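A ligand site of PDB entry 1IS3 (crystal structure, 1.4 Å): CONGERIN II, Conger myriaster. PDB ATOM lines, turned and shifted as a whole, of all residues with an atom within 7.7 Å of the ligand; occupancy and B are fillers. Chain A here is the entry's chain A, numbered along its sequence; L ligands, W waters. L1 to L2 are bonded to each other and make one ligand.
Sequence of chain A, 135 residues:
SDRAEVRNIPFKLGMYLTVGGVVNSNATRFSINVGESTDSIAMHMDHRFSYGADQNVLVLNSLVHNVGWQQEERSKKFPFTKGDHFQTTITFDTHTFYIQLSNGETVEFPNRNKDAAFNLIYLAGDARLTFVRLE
The guanidinium group of Arg 74 lies within hydrogen-bond range of an oxygen (O2) of LIG L1 (3.2 Å). O1 of LG2 L2 lies within hydrogen-bond range of OH of Tyr 51, at 2.7 Å. An oxygen (O3) of LIG L1 sits at hydrogen-bond distance from the guanidinium group of Arg 48, 2.7 Å away. An oxygen (O3) of LIG L1 sits at hydrogen-bond distance from the side-chain carboxylate of Glu 72 (2.5 Å). ND2 of Asn 61 lies within hydrogen-bond range of O5 of LG2 L2, 2.8 Å away. NE2 of His 44 sits at hydrogen-bond distance from O3 of LG2 L2 (2.8 Å). NH1 of Arg 29 sits at hydrogen-bond distance from O2 of LG2 L2 (2.8 Å).
The side-chain carboxylate (OE1) of Glu 72 lies within salt-bridge range of the guanidinium group (NH2) of Arg 74 (2.9 Å). ND2 of Asn 61 lies within hydrogen-bond range of O of Gln 70 (2.9 Å). The backbone NH (N) of Asp 46 is in hydrogen-bond range of the backbone carbonyl oxygen (O) of Val 59 (2.8 Å). OD2 of Asp 46 is in salt-bridge range of NE of Arg 48. The side-chain carboxylate (OD2) of Asp 54 lies within salt-bridge range of the guanidinium group (NH2) of Arg 48. The side-chain amide oxygen (OD1) of Asn 33 lies within hydrogen-bond range of a ring nitrogen (ND1) of His 44 (2.8 Å). The side-chain carboxylate (OD2) of Asp 46 is in salt-bridge range of the guanidinium group (NH1) of Arg 29 (2.9 Å). The side-chain amide oxygen (OD1) of Asn 61 sits close to the backbone carbonyl oxygen (O) of Gln 71, at 3.2 Å.
OD2 of Asp 46 touches O3 of LG2 L2, 3.5 Å away. CE2 of Trp 69 touches C4 of LG2 L2, 3.8 Å away. Within 4 Å of the ligand: Arg 29, His 44, Asp 46, Arg 48, Tyr 51, Asn 61, Trp 69, Glu 72 and Arg 74. The nearest printed residue that does not touch the ligand is Val 59 (4.1 Å).
Water W2 lies within hydrogen-bond range of the side-chain carboxylate of Asp 54 (2.7 Å) and an oxygen (O2) of LIG L1 (2.9 Å).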
ATOM      1  N   ARG A  29      37.495  -5.861 -11.232  1.00  0.00           N
ATOM      2  CA  ARG A  29      36.422  -5.075 -10.619  1.00  0.00           C
ATOM      3  C   ARG A  29      37.013  -4.073  -9.629  1.00  0.00           C
ATOM      4  O   ARG A  29      38.127  -4.263  -9.118  1.00  0.00           O
ATOM      5  CB  ARG A  29      35.436  -5.999  -9.880  1.00  0.00           C
ATOM      6  CG  ARG A  29      36.155  -6.789  -8.800  1.00  0.00           C
ATOM      7  CD  ARG A  29      35.461  -7.998  -8.228  1.00  0.00           C
ATOM      8  NE  ARG A  29      34.417  -7.647  -7.313  1.00  0.00           N
ATOM      9  CZ  ARG A  29      34.254  -8.180  -6.091  1.00  0.00           C
ATOM     10  NH1 ARG A  29      33.220  -7.753  -5.389  1.00  0.00           N
ATOM     11  NH2 ARG A  29      35.048  -9.068  -5.508  1.00  0.00           N
ATOM     12  N   SER A  31      35.399  -1.168  -6.379  1.00  0.00           N
ATOM     13  CA  SER A  31      34.168  -0.628  -5.798  1.00  0.00           C
ATOM     14  C   SER A  31      34.366   0.708  -5.110  1.00  0.00           C
ATOM     15  O   SER A  31      35.484   0.975  -4.658  1.00  0.00           O
ATOM     16  CB  SER A  31      33.578  -1.620  -4.796  1.00  0.00           C
ATOM     17  OG  SER A  31      34.403  -1.985  -3.702  1.00  0.00           O
ATOM     18  N   ASN A  33      32.711   2.626  -1.792  1.00  0.00           N
ATOM     19  CA  ASN A  33      31.975   2.170  -0.603  1.00  0.00           C
ATOM     20  C   ASN A  33      31.731   3.339   0.360  1.00  0.00           C
ATOM     21  O   ASN A  33      32.677   4.100   0.595  1.00  0.00           O
ATOM     22  CB  ASN A  33      32.791   1.100   0.136  1.00  0.00           C
ATOM     23  CG  ASN A  33      33.072  -0.081  -0.754  1.00  0.00           C
ATOM     24  OD1 ASN A  33      32.205  -0.911  -0.938  1.00  0.00           O
ATOM     25  ND2 ASN A  33      34.230  -0.183  -1.412  1.00  0.00           N
ATOM     26  N   HIS A  44      27.563  -0.033  -1.323  1.00  0.00           N
ATOM     27  CA  HIS A  44      28.675  -0.639  -2.020  1.00  0.00           C
ATOM     28  C   HIS A  44      28.361  -0.552  -3.527  1.00  0.00           C
ATOM     29  O   HIS A  44      27.313  -1.072  -3.905  1.00  0.00           O
ATOM     30  CB  HIS A  44      28.816  -2.098  -1.578  1.00  0.00           C
ATOM     31  CG  HIS A  44      29.772  -2.979  -2.409  1.00  0.00           C
ATOM     32  ND1 HIS A  44      31.096  -2.999  -2.405  1.00  0.00           N
ATOM     33  CD2 HIS A  44      29.391  -4.027  -3.257  1.00  0.00           C
ATOM     34  CE1 HIS A  44      31.548  -3.975  -3.174  1.00  0.00           C
ATOM     35  NE2 HIS A  44      30.508  -4.586  -3.687  1.00  0.00           N
ATOM     36  N   MET A  45      29.176   0.038  -4.405  1.00  0.00           N
ATOM     37  CA  MET A  45      28.891   0.117  -5.828  1.00  0.00           C
ATOM     38  C   MET A  45      30.082  -0.585  -6.486  1.00  0.00           C
ATOM     39  O   MET A  45      31.216  -0.059  -6.538  1.00  0.00           O
ATOM     40  CB  MET A  45      28.827   1.571  -6.172  1.00  0.00           C
ATOM     41  CG  MET A  45      28.616   1.746  -7.636  1.00  0.00           C
ATOM     42  SD  MET A  45      28.668   3.524  -7.994  1.00  0.00           S
ATOM     43  CE  MET A  45      27.689   3.379  -9.440  1.00  0.00           C
ATOM     44  N   ASP A  46      29.884  -1.800  -6.980  1.00  0.00           N
ATOM     45  CA  ASP A  46      30.938  -2.580  -7.552  1.00  0.00           C
ATOM     46  C   ASP A  46      30.878  -2.489  -9.073  1.00  0.00           C
ATOM     47  O   ASP A  46      29.804  -2.564  -9.680  1.00  0.00           O
ATOM     48  CB  ASP A  46      30.781  -4.005  -7.058  1.00  0.00           C
ATOM     49  CG  ASP A  46      32.022  -4.855  -7.215  1.00  0.00           C
ATOM     50  OD1 ASP A  46      33.130  -4.335  -7.199  1.00  0.00           O
ATOM     51  OD2 ASP A  46      31.897  -6.063  -7.350  1.00  0.00           O
ATOM     52  N   HIS A  47      32.029  -2.286  -9.699  1.00  0.00           N
ATOM     53  CA  HIS A  47      32.142  -2.070 -11.131  1.00  0.00           C
ATOM     54  C   HIS A  47      32.815  -3.320 -11.657  1.00  0.00           C
ATOM     55  O   HIS A  47      34.017  -3.505 -11.421  1.00  0.00           O
ATOM     56  CB  HIS A  47      33.015  -0.832 -11.461  1.00  0.00           C
ATOM     57  CG  HIS A  47      32.578   0.441 -10.769  1.00  0.00           C
ATOM     58  ND1 HIS A  47      32.636   0.686  -9.446  1.00  0.00           N
ATOM     59  CD2 HIS A  47      32.146   1.576 -11.393  1.00  0.00           C
ATOM     60  CE1 HIS A  47      32.260   1.932  -9.239  1.00  0.00           C
ATOM     61  NE2 HIS A  47      31.978   2.447 -10.417  1.00  0.00           N
ATOM     62  N   ARG A  48      32.057  -4.200 -12.321  1.00  0.00           N
ATOM     63  CA  ARG A  48      32.605  -5.509 -12.695  1.00  0.00           C
ATOM     64  C   ARG A  48      32.905  -5.598 -14.175  1.00  0.00           C
ATOM     65  O   ARG A  48      31.983  -5.592 -15.007  1.00  0.00           O
ATOM     66  CB  ARG A  48      31.618  -6.596 -12.314  1.00  0.00           C
ATOM     67  CG  ARG A  48      31.470  -6.729 -10.791  1.00  0.00           C
ATOM     68  CD  ARG A  48      30.348  -7.685 -10.374  1.00  0.00           C
ATOM     69  NE  ARG A  48      30.206  -7.705  -8.904  1.00  0.00           N
ATOM     70  CZ  ARG A  48      29.501  -8.596  -8.195  1.00  0.00           C
ATOM     71  NH1 ARG A  48      29.435  -8.523  -6.855  1.00  0.00           N
ATOM     72  NH2 ARG A  48      28.836  -9.541  -8.836  1.00  0.00           N
ATOM     73  N   TYR A  51      33.939 -10.694 -13.534  1.00  0.00           N
ATOM     74  CA  TYR A  51      33.886 -11.269 -12.208  1.00  0.00           C
ATOM     75  C   TYR A  51      32.857 -12.365 -12.256  1.00  0.00           C
ATOM     76  O   TYR A  51      31.659 -12.095 -12.322  1.00  0.00           O
ATOM     77  CB  TYR A  51      33.483 -10.187 -11.158  1.00  0.00           C
ATOM     78  CG  TYR A  51      33.326 -10.735  -9.740  1.00  0.00           C
ATOM     79  CD1 TYR A  51      34.426 -11.247  -9.050  1.00  0.00           C
ATOM     80  CD2 TYR A  51      32.074 -10.723  -9.134  1.00  0.00           C
ATOM     81  CE1 TYR A  51      34.282 -11.740  -7.751  1.00  0.00           C
ATOM     82  CE2 TYR A  51      31.916 -11.202  -7.833  1.00  0.00           C
ATOM     83  CZ  TYR A  51      33.032 -11.711  -7.149  1.00  0.00           C
ATOM     84  OH  TYR A  51      32.855 -12.165  -5.854  1.00  0.00           O
ATOM     85  N   ALA A  53      30.356 -14.728 -13.665  1.00  0.00           N
ATOM     86  CA  ALA A  53      29.598 -14.567 -14.889  1.00  0.00           C
ATOM     87  C   ALA A  53      29.309 -13.119 -15.189  1.00  0.00           C
ATOM     88  O   ALA A  53      28.660 -12.856 -16.195  1.00  0.00           O
ATOM     89  CB  ALA A  53      28.245 -15.248 -14.817  1.00  0.00           C
ATOM     90  N   ASP A  54      29.687 -12.161 -14.345  1.00  0.00           N
ATOM     91  CA  ASP A  54      29.411 -10.750 -14.567  1.00  0.00           C
ATOM     92  C   ASP A  54      30.454 -10.045 -15.399  1.00  0.00           C
ATOM     93  O   ASP A  54      31.657 -10.080 -15.079  1.00  0.00           O
ATOM     94  CB  ASP A  54      29.311 -10.052 -13.218  1.00  0.00           C
ATOM     95  CG  ASP A  54      28.022 -10.394 -12.487  1.00  0.00           C
ATOM     96  OD1 ASP A  54      26.998 -10.511 -13.153  1.00  0.00           O
ATOM     97  OD2 ASP A  54      28.023 -10.512 -11.273  1.00  0.00           O
ATOM     98  N   VAL A  59      26.996  -3.548  -9.736  1.00  0.00           N
ATOM     99  CA  VAL A  59      26.243  -4.276  -8.729  1.00  0.00           C
ATOM    100  C   VAL A  59      26.249  -3.401  -7.468  1.00  0.00           C
ATOM    101  O   VAL A  59      27.327  -2.977  -6.997  1.00  0.00           O
ATOM    102  CB  VAL A  59      26.906  -5.651  -8.471  1.00  0.00           C
ATOM    103  CG1 VAL A  59      26.189  -6.401  -7.328  1.00  0.00           C
ATOM    104  CG2 VAL A  59      26.827  -6.499  -9.754  1.00  0.00           C
ATOM    105  N   LEU A  60      25.071  -3.106  -6.915  1.00  0.00           N
ATOM    106  CA  LEU A  60      24.934  -2.299  -5.712  1.00  0.00           C
ATOM    107  C   LEU A  60      24.363  -3.115  -4.554  1.00  0.00           C
ATOM    108  O   LEU A  60      23.462  -3.950  -4.750  1.00  0.00           O
ATOM    109  CB  LEU A  60      24.025  -1.103  -5.990  1.00  0.00           C
ATOM    110  CG  LEU A  60      24.672  -0.140  -6.988  1.00  0.00           C
ATOM    111  CD1 LEU A  60      24.184  -0.474  -8.392  1.00  0.00           C
ATOM    112  CD2 LEU A  60      24.338   1.273  -6.600  1.00  0.00           C
ATOM    113  N   ASN A  61      24.890  -2.908  -3.347  1.00  0.00           N
ATOM    114  CA  ASN A  61      24.410  -3.644  -2.187  1.00  0.00           C
ATOM    115  C   ASN A  61      24.837  -3.003  -0.877  1.00  0.00           C
ATOM    116  O   ASN A  61      25.563  -1.995  -0.896  1.00  0.00           O
ATOM    117  CB  ASN A  61      24.929  -5.102  -2.261  1.00  0.00           C
ATOM    118  CG  ASN A  61      24.040  -6.151  -1.579  1.00  0.00           C
ATOM    119  OD1 ASN A  61      23.148  -5.844  -0.806  1.00  0.00           O
ATOM    120  ND2 ASN A  61      24.277  -7.424  -1.793  1.00  0.00           N
ATOM    121  N   SER A  62      24.334  -3.474   0.262  1.00  0.00           N
ATOM    122  CA  SER A  62      24.765  -3.030   1.571  1.00  0.00           C
ATOM    123  C   SER A  62      25.307  -4.264   2.286  1.00  0.00           C
ATOM    124  O   SER A  62      24.897  -5.421   2.023  1.00  0.00           O
ATOM    125  CB  SER A  62      23.570  -2.424   2.278  1.00  0.00           C
ATOM    126  OG  SER A  62      22.527  -3.392   2.367  1.00  0.00           O
ATOM    127  N   LEU A  63      26.211  -3.997   3.213  1.00  0.00           N
ATOM    128  CA  LEU A  63      26.884  -4.989   4.009  1.00  0.00           C
ATOM    129  C   LEU A  63      26.623  -4.639   5.450  1.00  0.00           C
ATOM    130  O   LEU A  63      26.899  -3.493   5.860  1.00  0.00           O
ATOM    131  CB  LEU A  63      28.397  -4.958   3.752  1.00  0.00           C
ATOM    132  CG  LEU A  63      29.277  -5.896   4.551  1.00  0.00           C
ATOM    133  CD1 LEU A  63      28.984  -7.342   4.227  1.00  0.00           C
ATOM    134  CD2 LEU A  63      30.716  -5.640   4.176  1.00  0.00           C
ATOM    135  N   TRP A  69      26.091  -9.537   3.253  1.00  0.00           N
ATOM    136  CA  TRP A  69      25.527  -8.828   2.128  1.00  0.00           C
ATOM    137  C   TRP A  69      24.022  -9.002   2.050  1.00  0.00           C
ATOM    138  O   TRP A  69      23.525 -10.093   2.346  1.00  0.00           O
ATOM    139  CB  TRP A  69      26.218  -9.327   0.829  1.00  0.00           C
ATOM    140  CG  TRP A  69      27.678  -8.863   0.722  1.00  0.00           C
ATOM    141  CD1 TRP A  69      28.723  -9.725   0.940  1.00  0.00           C
ATOM    142  CD2 TRP A  69      28.126  -7.568   0.482  1.00  0.00           C
ATOM    143  NE1 TRP A  69      29.830  -9.005   0.835  1.00  0.00           N
ATOM    144  CE2 TRP A  69      29.525  -7.721   0.565  1.00  0.00           C
ATOM    145  CE3 TRP A  69      27.564  -6.303   0.209  1.00  0.00           C
ATOM    146  CZ2 TRP A  69      30.353  -6.589   0.380  1.00  0.00           C
ATOM    147  CZ3 TRP A  69      28.395  -5.199   0.036  1.00  0.00           C
ATOM    148  CH2 TRP A  69      29.780  -5.351   0.115  1.00  0.00           C
ATOM    149  N   GLN A  70      23.302  -7.947   1.691  1.00  0.00           N
ATOM    150  CA  GLN A  70      21.856  -7.959   1.616  1.00  0.00           C
ATOM    151  C   GLN A  70      21.413  -8.212   0.169  1.00  0.00           C
ATOM    152  O   GLN A  70      22.109  -8.958  -0.537  1.00  0.00           O
ATOM    153  CB  GLN A  70      21.360  -6.618   2.186  1.00  0.00           C
ATOM    154  CG  GLN A  70      21.790  -6.526   3.675  1.00  0.00           C
ATOM    155  CD  GLN A  70      21.399  -7.744   4.543  1.00  0.00           C
ATOM    156  OE1 GLN A  70      20.215  -8.033   4.722  1.00  0.00           O
ATOM    157  NE2 GLN A  70      22.346  -8.500   5.100  1.00  0.00           N
ATOM    158  N   GLN A  71      20.299  -7.667  -0.298  1.00  0.00           N
ATOM    159  CA  GLN A  71      19.802  -7.960  -1.632  1.00  0.00           C
ATOM    160  C   GLN A  71      20.540  -7.073  -2.657  1.00  0.00           C
ATOM    161  O   GLN A  71      20.530  -5.841  -2.562  1.00  0.00           O
ATOM    162  CB  GLN A  71      18.310  -7.702  -1.587  1.00  0.00           C
ATOM    163  CG  GLN A  71      17.552  -7.953  -2.868  1.00  0.00           C
ATOM    164  CD  GLN A  71      16.731  -6.764  -3.425  1.00  0.00           C
ATOM    165  OE1 GLN A  71      15.597  -6.451  -3.009  1.00  0.00           O
ATOM    166  NE2 GLN A  71      17.247  -6.062  -4.455  1.00  0.00           N
ATOM    167  N   GLU A  72      21.189  -7.677  -3.654  1.00  0.00           N
ATOM    168  CA  GLU A  72      21.857  -6.954  -4.755  1.00  0.00           C
ATOM    169  C   GLU A  72      20.902  -6.263  -5.709  1.00  0.00           C
ATOM    170  O   GLU A  72      19.819  -6.798  -6.014  1.00  0.00           O
ATOM    171  CB  GLU A  72      22.648  -7.820  -5.705  1.00  0.00           C
ATOM    172  CG  GLU A  72      23.617  -8.696  -5.034  1.00  0.00           C
ATOM    173  CD  GLU A  72      24.491  -9.461  -5.998  1.00  0.00           C
ATOM    174  OE1 GLU A  72      24.087  -9.811  -7.116  1.00  0.00           O
ATOM    175  OE2 GLU A  72      25.600  -9.717  -5.593  1.00  0.00           O
ATOM    176  N   GLU A  73      21.289  -5.105  -6.211  1.00  0.00           N
ATOM    177  CA  GLU A  73      20.582  -4.419  -7.275  1.00  0.00           C
ATOM    178  C   GLU A  73      21.617  -4.314  -8.364  1.00  0.00           C
ATOM    179  O   GLU A  73      22.809  -4.183  -8.081  1.00  0.00           O
ATOM    180  CB  GLU A  73      20.139  -3.055  -6.815  1.00  0.00           C
ATOM    181  CG  GLU A  73      18.878  -3.368  -5.964  1.00  0.00           C
ATOM    182  CD  GLU A  73      17.997  -2.227  -5.475  1.00  0.00           C
ATOM    183  OE1 GLU A  73      17.286  -2.423  -4.463  1.00  0.00           O
ATOM    184  OE2 GLU A  73      18.008  -1.154  -6.098  1.00  0.00           O
ATOM    185  N   ARG A  74      21.219  -4.515  -9.610  1.00  0.00           N
ATOM    186  CA  ARG A  74      22.151  -4.467 -10.741  1.00  0.00           C
ATOM    187  C   ARG A  74      21.806  -3.440 -11.797  1.00  0.00           C
ATOM    188  O   ARG A  74      20.627  -3.121 -11.984  1.00  0.00           O
ATOM    189  CB  ARG A  74      22.225  -5.829 -11.407  1.00  0.00           C
ATOM    190  CG  ARG A  74      22.950  -6.809 -10.502  1.00  0.00           C
ATOM    191  CD  ARG A  74      22.562  -8.267 -10.691  1.00  0.00           C
ATOM    192  NE  ARG A  74      23.424  -9.137  -9.892  1.00  0.00           N
ATOM    193  CZ  ARG A  74      24.612  -9.529 -10.391  1.00  0.00           C
ATOM    194  NH1 ARG A  74      25.000  -9.140 -11.607  1.00  0.00           N
ATOM    195  NH2 ARG A  74      25.419 -10.317  -9.675  1.00  0.00           N
HETATM  196  C1  LIG L   1      26.463 -13.060  -6.769  1.00  0.00           C
HETATM  197  C2  LIG L   1      27.696 -12.167  -6.622  1.00  0.00           C
HETATM  198  C3  LIG L   1      28.220 -12.260  -5.191  1.00  0.00           C
HETATM  199  C4  LIG L   1      28.507 -13.731  -4.835  1.00  0.00           C
HETATM  200  C5  LIG L   1      28.912 -13.920  -3.388  1.00  0.00           C
HETATM  201  C6  LIG L   1      26.847 -14.493  -6.380  1.00  0.00           C
HETATM  202  O1  LIG L   1      25.728 -15.303  -6.472  1.00  0.00           O
HETATM  203  O2  LIG L   1      25.992 -13.023  -8.107  1.00  0.00           O
HETATM  204  O3  LIG L   1      27.368 -10.830  -6.933  1.00  0.00           O
HETATM  205  O4  LIG L   1      29.438 -11.509  -5.073  1.00  0.00           O
HETATM  206  O5  LIG L   1      27.308 -14.526  -5.033  1.00  0.00           O
HETATM  207  O6  LIG L   1      27.937 -13.394  -2.506  1.00  0.00           O
HETATM  208  C1  LG2 L   2      29.532 -10.622  -4.005  1.00  0.00           C
HETATM  209  C2  LG2 L   2      30.987 -10.175  -3.874  1.00  0.00           C
HETATM  210  C3  LG2 L   2      31.122  -9.085  -2.835  1.00  0.00           C
HETATM  211  C4  LG2 L   2      30.149  -7.939  -3.130  1.00  0.00           C
HETATM  212  C5  LG2 L   2      28.734  -8.505  -3.241  1.00  0.00           C
HETATM  213  C6  LG2 L   2      27.712  -7.449  -3.564  1.00  0.00           C
HETATM  214  O1  LG2 L   2      31.784 -11.280  -3.513  1.00  0.00           O
HETATM  215  O2  LG2 L   2      32.456  -8.591  -2.821  1.00  0.00           O
HETATM  216  O3  LG2 L   2      30.497  -7.275  -4.335  1.00  0.00           O
HETATM  217  O4  LG2 L   2      28.679  -9.498  -4.285  1.00  0.00           O
HETATM  218  O5  LG2 L   2      26.412  -8.008  -3.583  1.00  0.00           O
HETATM  219  O   HOH W   1      32.132 -13.743  -1.297  1.00  0.00           O
HETATM  220  O   HOH W   2      28.247 -12.840  -9.998  1.00  0.00           O
